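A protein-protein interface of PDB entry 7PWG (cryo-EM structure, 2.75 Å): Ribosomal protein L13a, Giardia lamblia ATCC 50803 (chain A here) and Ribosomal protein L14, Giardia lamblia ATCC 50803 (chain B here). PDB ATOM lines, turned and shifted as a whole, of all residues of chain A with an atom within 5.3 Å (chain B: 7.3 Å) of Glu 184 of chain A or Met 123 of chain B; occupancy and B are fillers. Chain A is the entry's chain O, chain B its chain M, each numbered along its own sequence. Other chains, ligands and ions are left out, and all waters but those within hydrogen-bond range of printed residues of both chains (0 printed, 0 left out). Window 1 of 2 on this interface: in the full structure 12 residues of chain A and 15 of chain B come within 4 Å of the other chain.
Among the printed residues, pairs that only touch across the chains: Ile 175 of chain A with Ile 126 of chain B (3.98 Å), Ile 175 of chain A with Ala 127 of chain B (3.6 Å), Ala 178 of chain A with Ile 126 of chain B (3.6 Å), Lys 181 of chain A with Arg 125 of chain B (3.6 Å), Lys 181 of chain A with Ile 126 of chain B (3.8 Å), Glu 184 of chain A with Ile 126 of chain B (3.97 Å), Arg 187 of chain A with Glu 118 of chain B (3.4 Å), Arg 187 of chain A with Ala 122 of chain B (3.2 Å) and Ile 188 of chain A with Arg 119 of chain B (3.2 Å).
The backbone carbonyl oxygen (O) of Ala 183 of chain A sits close to the guanidinium group (NE) of Arg 187 of chain A (3.3 Å).
The side-chain sulfur (SD) of Met 123 of chain B sits close to the side-chain carboxylate (OE2) of Glu 184 of chain A (3.0 Å).
Printed residues of chain A that touch a printed residue of chain B: Ile 175, Ala 178, Lys 181, Glu 184, Arg 187 and Ile 188. Of the 11 printed residues of chain B, 7 touch a printed residue of chain A. Along chain B the printed residues that touch a printed residue of chain A span positions 118 to 127.
Glu 184 of chain A touches just these residues of chain B: Met 123 (3.0 Å) and Ile 126 (3.97 Å). Met 123 of chain B touches just one residue of chain A: Glu 184. Printed residues of chain B within 4 Å of Ala 178 of chain A: Ile 126 (3.6 Å). Of the printed residues of chain B, Lys 181 of chain A touches Arg 125 and Ile 126. Of the printed residues of chain A, Ala 127 of chain B touches Ile 175 (3.6 Å). Of the printed residues of chain B, Ile 175 of chain A touches Ile 126 and Ala 127. Printed residues of chain A within 4 Å of Arg 119 of chain B: Ile 188 (3.2 Å). Met 121 of chain B touches none of the printed residues of chain A.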
ATOM      1  N   ILE A 175       6.043 -26.638 -24.347  1.00  0.00           N
ATOM      2  CA  ILE A 175       6.836 -25.420 -24.216  1.00  0.00           C
ATOM      3  C   ILE A 175       6.802 -24.636 -25.517  1.00  0.00           C
ATOM      4  O   ILE A 175       6.613 -23.417 -25.521  1.00  0.00           O
ATOM      5  CB  ILE A 175       8.286 -25.755 -23.816  1.00  0.00           C
ATOM      6  CG1 ILE A 175       8.347 -26.512 -22.489  1.00  0.00           C
ATOM      7  CG2 ILE A 175       9.138 -24.505 -23.776  1.00  0.00           C
ATOM      8  CD1 ILE A 175       8.029 -25.702 -21.290  1.00  0.00           C
ATOM      9  N   ALA A 178       3.850 -22.347 -27.224  1.00  0.00           N
ATOM     10  CA  ALA A 178       3.631 -20.956 -26.862  1.00  0.00           C
ATOM     11  C   ALA A 178       3.992 -20.008 -27.998  1.00  0.00           C
ATOM     12  O   ALA A 178       4.989 -19.285 -27.930  1.00  0.00           O
ATOM     13  CB  ALA A 178       4.422 -20.616 -25.603  1.00  0.00           C
ATOM     14  N   LYS A 181       1.729 -16.047 -26.881  1.00  0.00           N
ATOM     15  CA  LYS A 181       2.158 -14.917 -26.063  1.00  0.00           C
ATOM     16  C   LYS A 181       2.641 -13.838 -27.024  1.00  0.00           C
ATOM     17  O   LYS A 181       3.755 -13.916 -27.551  1.00  0.00           O
ATOM     18  CB  LYS A 181       3.236 -15.337 -25.067  1.00  0.00           C
ATOM     19  CG  LYS A 181       3.698 -14.243 -24.111  1.00  0.00           C
ATOM     20  CD  LYS A 181       4.459 -14.813 -22.910  1.00  0.00           C
ATOM     21  CE  LYS A 181       5.337 -13.762 -22.219  1.00  0.00           C
ATOM     22  NZ  LYS A 181       5.992 -14.238 -20.962  1.00  0.00           N
ATOM     23  N   ASP A 182       1.774 -12.853 -27.283  1.00  0.00           N
ATOM     24  CA  ASP A 182       2.098 -11.822 -28.263  1.00  0.00           C
ATOM     25  C   ASP A 182       3.308 -11.016 -27.819  1.00  0.00           C
ATOM     26  O   ASP A 182       4.187 -10.714 -28.629  1.00  0.00           O
ATOM     27  CB  ASP A 182       0.891 -10.903 -28.496  1.00  0.00           C
ATOM     28  CG  ASP A 182       1.044 -10.012 -29.740  1.00  0.00           C
ATOM     29  OD1 ASP A 182       2.174  -9.571 -30.056  1.00  0.00           O
ATOM     30  OD2 ASP A 182       0.020  -9.757 -30.418  1.00  0.00           O
ATOM     31  N   ALA A 183       3.391 -10.702 -26.527  1.00  0.00           N
ATOM     32  CA  ALA A 183       4.499  -9.925 -25.992  1.00  0.00           C
ATOM     33  C   ALA A 183       5.856 -10.543 -26.307  1.00  0.00           C
ATOM     34  O   ALA A 183       6.885  -9.921 -26.024  1.00  0.00           O
ATOM     35  CB  ALA A 183       4.322  -9.758 -24.486  1.00  0.00           C
ATOM     36  N   GLU A 184       5.877 -11.751 -26.864  1.00  0.00           N
ATOM     37  CA  GLU A 184       7.051 -12.326 -27.503  1.00  0.00           C
ATOM     38  C   GLU A 184       7.006 -12.235 -29.021  1.00  0.00           C
ATOM     39  O   GLU A 184       8.052 -12.076 -29.658  1.00  0.00           O
ATOM     40  CB  GLU A 184       7.192 -13.788 -27.093  1.00  0.00           C
ATOM     41  CG  GLU A 184       8.249 -14.524 -27.812  1.00  0.00           C
ATOM     42  CD  GLU A 184       8.308 -15.948 -27.376  1.00  0.00           C
ATOM     43  OE1 GLU A 184       7.324 -16.674 -27.609  1.00  0.00           O
ATOM     44  OE2 GLU A 184       9.328 -16.325 -26.781  1.00  0.00           O
ATOM     45  N   LEU A 185       5.818 -12.327 -29.617  1.00  0.00           N
ATOM     46  CA  LEU A 185       5.691 -12.092 -31.048  1.00  0.00           C
ATOM     47  C   LEU A 185       6.040 -10.663 -31.402  1.00  0.00           C
ATOM     48  O   LEU A 185       6.250 -10.357 -32.576  1.00  0.00           O
ATOM     49  CB  LEU A 185       4.280 -12.433 -31.519  1.00  0.00           C
ATOM     50  CG  LEU A 185       3.851 -13.850 -31.148  1.00  0.00           C
ATOM     51  CD1 LEU A 185       2.548 -14.224 -31.824  1.00  0.00           C
ATOM     52  CD2 LEU A 185       4.959 -14.833 -31.513  1.00  0.00           C
ATOM     53  N   GLN A 186       6.090  -9.782 -30.414  1.00  0.00           N
ATOM     54  CA  GLN A 186       6.664  -8.469 -30.614  1.00  0.00           C
ATOM     55  C   GLN A 186       8.177  -8.494 -30.468  1.00  0.00           C
ATOM     56  O   GLN A 186       8.852  -7.613 -31.004  1.00  0.00           O
ATOM     57  CB  GLN A 186       6.018  -7.478 -29.639  1.00  0.00           C
ATOM     58  CG  GLN A 186       6.820  -7.165 -28.393  1.00  0.00           C
ATOM     59  CD  GLN A 186       7.349  -5.745 -28.399  1.00  0.00           C
ATOM     60  OE1 GLN A 186       6.842  -4.895 -29.128  1.00  0.00           O
ATOM     61  NE2 GLN A 186       8.386  -5.487 -27.610  1.00  0.00           N
ATOM     62  N   ARG A 187       8.725  -9.500 -29.781  1.00  0.00           N
ATOM     63  CA  ARG A 187      10.173  -9.653 -29.696  1.00  0.00           C
ATOM     64  C   ARG A 187      10.756 -10.325 -30.936  1.00  0.00           C
ATOM     65  O   ARG A 187      11.808  -9.912 -31.422  1.00  0.00           O
ATOM     66  CB  ARG A 187      10.546 -10.446 -28.443  1.00  0.00           C
ATOM     67  CG  ARG A 187      10.654  -9.607 -27.195  1.00  0.00           C
ATOM     68  CD  ARG A 187      10.130 -10.330 -25.974  1.00  0.00           C
ATOM     69  NE  ARG A 187       9.920  -9.392 -24.874  1.00  0.00           N
ATOM     70  CZ  ARG A 187       9.387  -9.692 -23.688  1.00  0.00           C
ATOM     71  NH1 ARG A 187       8.992 -10.929 -23.412  1.00  0.00           N
ATOM     72  NH2 ARG A 187       9.246  -8.738 -22.770  1.00  0.00           N
ATOM     73  N   ILE A 188      10.090 -11.350 -31.466  1.00  0.00           N
ATOM     74  CA  ILE A 188      10.657 -12.120 -32.574  1.00  0.00           C
ATOM     75  C   ILE A 188      10.698 -11.291 -33.851  1.00  0.00           C
ATOM     76  O   ILE A 188      11.635 -11.396 -34.647  1.00  0.00           O
ATOM     77  CB  ILE A 188       9.866 -13.423 -32.773  1.00  0.00           C
ATOM     78  CG1 ILE A 188       9.889 -14.259 -31.501  1.00  0.00           C
ATOM     79  CG2 ILE A 188      10.439 -14.245 -33.916  1.00  0.00           C
ATOM     80  CD1 ILE A 188      11.229 -14.400 -30.907  1.00  0.00           C
ATOM     81  N   ASN A 189       9.681 -10.466 -34.073  1.00  0.00           N
ATOM     82  CA  ASN A 189       9.595  -9.709 -35.317  1.00  0.00           C
ATOM     83  C   ASN A 189      10.601  -8.564 -35.373  1.00  0.00           C
ATOM     84  O   ASN A 189      11.005  -8.158 -36.466  1.00  0.00           O
ATOM     85  CB  ASN A 189       8.176  -9.191 -35.494  1.00  0.00           C
ATOM     86  CG  ASN A 189       7.161 -10.311 -35.575  1.00  0.00           C
ATOM     87  OD1 ASN A 189       7.403 -11.328 -36.221  1.00  0.00           O
ATOM     88  ND2 ASN A 189       6.018 -10.135 -34.917  1.00  0.00           N
ATOM     89  N   GLU B 118      15.447  -9.970 -23.901  1.00  0.00           N
ATOM     90  CA  GLU B 118      14.004 -10.128 -23.787  1.00  0.00           C
ATOM     91  C   GLU B 118      13.548 -11.514 -24.230  1.00  0.00           C
ATOM     92  O   GLU B 118      12.539 -12.015 -23.732  1.00  0.00           O
ATOM     93  CB  GLU B 118      13.275  -9.057 -24.598  1.00  0.00           C
ATOM     94  CG  GLU B 118      13.857  -7.657 -24.509  1.00  0.00           C
ATOM     95  CD  GLU B 118      14.102  -7.207 -23.093  1.00  0.00           C
ATOM     96  OE1 GLU B 118      15.261  -6.876 -22.760  1.00  0.00           O
ATOM     97  OE2 GLU B 118      13.129  -7.182 -22.306  1.00  0.00           O
ATOM     98  N   ARG B 119      14.257 -12.142 -25.172  1.00  0.00           N
ATOM     99  CA  ARG B 119      13.878 -13.488 -25.592  1.00  0.00           C
ATOM    100  C   ARG B 119      14.261 -14.520 -24.544  1.00  0.00           C
ATOM    101  O   ARG B 119      13.501 -15.456 -24.288  1.00  0.00           O
ATOM    102  CB  ARG B 119      14.509 -13.843 -26.936  1.00  0.00           C
ATOM    103  CG  ARG B 119      14.044 -15.170 -27.483  1.00  0.00           C
ATOM    104  CD  ARG B 119      14.845 -15.593 -28.705  1.00  0.00           C
ATOM    105  NE  ARG B 119      14.208 -15.195 -29.948  1.00  0.00           N
ATOM    106  CZ  ARG B 119      14.869 -14.859 -31.045  1.00  0.00           C
ATOM    107  NH1 ARG B 119      14.213 -14.509 -32.136  1.00  0.00           N
ATOM    108  NH2 ARG B 119      16.189 -14.856 -31.049  1.00  0.00           N
ATOM    109  N   LYS B 120      15.427 -14.359 -23.922  1.00  0.00           N
ATOM    110  CA  LYS B 120      15.860 -15.303 -22.900  1.00  0.00           C
ATOM    111  C   LYS B 120      14.921 -15.313 -21.701  1.00  0.00           C
ATOM    112  O   LYS B 120      14.691 -16.369 -21.104  1.00  0.00           O
ATOM    113  CB  LYS B 120      17.284 -14.978 -22.454  1.00  0.00           C
ATOM    114  CG  LYS B 120      17.768 -15.838 -21.314  1.00  0.00           C
ATOM    115  CD  LYS B 120      18.987 -15.277 -20.616  1.00  0.00           C
ATOM    116  CE  LYS B 120      20.255 -15.823 -21.224  1.00  0.00           C
ATOM    117  NZ  LYS B 120      21.456 -15.537 -20.404  1.00  0.00           N
ATOM    118  N   MET B 121      14.375 -14.156 -21.333  1.00  0.00           N
ATOM    119  CA  MET B 121      13.514 -14.043 -20.165  1.00  0.00           C
ATOM    120  C   MET B 121      12.047 -14.282 -20.473  1.00  0.00           C
ATOM    121  O   MET B 121      11.261 -14.500 -19.547  1.00  0.00           O
ATOM    122  CB  MET B 121      13.673 -12.657 -19.533  1.00  0.00           C
ATOM    123  CG  MET B 121      15.106 -12.290 -19.214  1.00  0.00           C
ATOM    124  SD  MET B 121      15.819 -13.385 -17.993  1.00  0.00           S
ATOM    125  CE  MET B 121      14.590 -13.222 -16.713  1.00  0.00           C
ATOM    126  N   ALA B 122      11.647 -14.198 -21.736  1.00  0.00           N
ATOM    127  CA  ALA B 122      10.293 -14.588 -22.095  1.00  0.00           C
ATOM    128  C   ALA B 122      10.148 -16.100 -22.104  1.00  0.00           C
ATOM    129  O   ALA B 122       9.188 -16.646 -21.551  1.00  0.00           O
ATOM    130  CB  ALA B 122       9.922 -14.005 -23.455  1.00  0.00           C
ATOM    131  N   MET B 123      11.113 -16.794 -22.709  1.00  0.00           N
ATOM    132  CA  MET B 123      11.061 -18.242 -22.785  1.00  0.00           C
ATOM    133  C   MET B 123      11.193 -18.895 -21.424  1.00  0.00           C
ATOM    134  O   MET B 123      10.859 -20.073 -21.286  1.00  0.00           O
ATOM    135  CB  MET B 123      12.144 -18.763 -23.726  1.00  0.00           C
ATOM    136  CG  MET B 123      11.841 -18.530 -25.187  1.00  0.00           C
ATOM    137  SD  MET B 123      10.144 -18.953 -25.621  1.00  0.00           S
ATOM    138  CE  MET B 123      10.079 -20.705 -25.231  1.00  0.00           C
ATOM    139  N   LYS B 124      11.662 -18.164 -20.419  1.00  0.00           N
ATOM    140  CA  LYS B 124      11.610 -18.652 -19.048  1.00  0.00           C
ATOM    141  C   LYS B 124      10.301 -18.296 -18.352  1.00  0.00           C
ATOM    142  O   LYS B 124       9.827 -19.069 -17.517  1.00  0.00           O
ATOM    143  CB  LYS B 124      12.802 -18.112 -18.257  1.00  0.00           C
ATOM    144  CG  LYS B 124      12.994 -18.770 -16.921  1.00  0.00           C
ATOM    145  CD  LYS B 124      14.114 -18.120 -16.140  1.00  0.00           C
ATOM    146  CE  LYS B 124      15.471 -18.440 -16.731  1.00  0.00           C
ATOM    147  NZ  LYS B 124      16.566 -17.975 -15.842  1.00  0.00           N
ATOM    148  N   ARG B 125       9.696 -17.155 -18.673  1.00  0.00           N
ATOM    149  CA  ARG B 125       8.359 -16.834 -18.178  1.00  0.00           C
ATOM    150  C   ARG B 125       7.269 -17.587 -18.925  1.00  0.00           C
ATOM    151  O   ARG B 125       6.089 -17.277 -18.743  1.00  0.00           O
ATOM    152  CB  ARG B 125       8.107 -15.322 -18.251  1.00  0.00           C
ATOM    153  CG  ARG B 125       8.625 -14.568 -17.022  1.00  0.00           C
ATOM    154  CD  ARG B 125       8.563 -13.043 -17.118  1.00  0.00           C
ATOM    155  NE  ARG B 125       8.363 -12.444 -15.800  1.00  0.00           N
ATOM    156  CZ  ARG B 125       8.203 -11.143 -15.555  1.00  0.00           C
ATOM    157  NH1 ARG B 125       8.215 -10.256 -16.545  1.00  0.00           N
ATOM    158  NH2 ARG B 125       8.024 -10.733 -14.306  1.00  0.00           N
ATOM    159  N   ILE B 126       7.645 -18.550 -19.765  1.00  0.00           N
ATOM    160  CA  ILE B 126       6.715 -19.444 -20.433  1.00  0.00           C
ATOM    161  C   ILE B 126       6.885 -20.881 -19.959  1.00  0.00           C
ATOM    162  O   ILE B 126       5.899 -21.596 -19.769  1.00  0.00           O
ATOM    163  CB  ILE B 126       6.896 -19.356 -21.964  1.00  0.00           C
ATOM    164  CG1 ILE B 126       6.041 -18.245 -22.558  1.00  0.00           C
ATOM    165  CG2 ILE B 126       6.600 -20.690 -22.627  1.00  0.00           C
ATOM    166  CD1 ILE B 126       6.286 -18.033 -24.022  1.00  0.00           C
ATOM    167  N   ALA B 127       8.133 -21.325 -19.787  1.00  0.00           N
ATOM    168  CA  ALA B 127       8.405 -22.704 -19.410  1.00  0.00           C
ATOM    169  C   ALA B 127       7.942 -23.024 -17.999  1.00  0.00           C
ATOM    170  O   ALA B 127       7.761 -24.202 -17.677  1.00  0.00           O
ATOM    171  CB  ALA B 127       9.894 -23.004 -19.548  1.00  0.00           C
ATOM    172  N   MET B 128       7.751 -22.014 -17.152  1.00  0.00           N
ATOM    173  CA  MET B 128       7.102 -22.196 -15.857  1.00  0.00           C
ATOM    174  C   MET B 128       5.584 -22.219 -16.044  1.00  0.00           C
ATOM    175  O   MET B 128       4.830 -21.508 -15.383  1.00  0.00           O
ATOM    176  CB  MET B 128       7.524 -21.097 -14.890  1.00  0.00           C
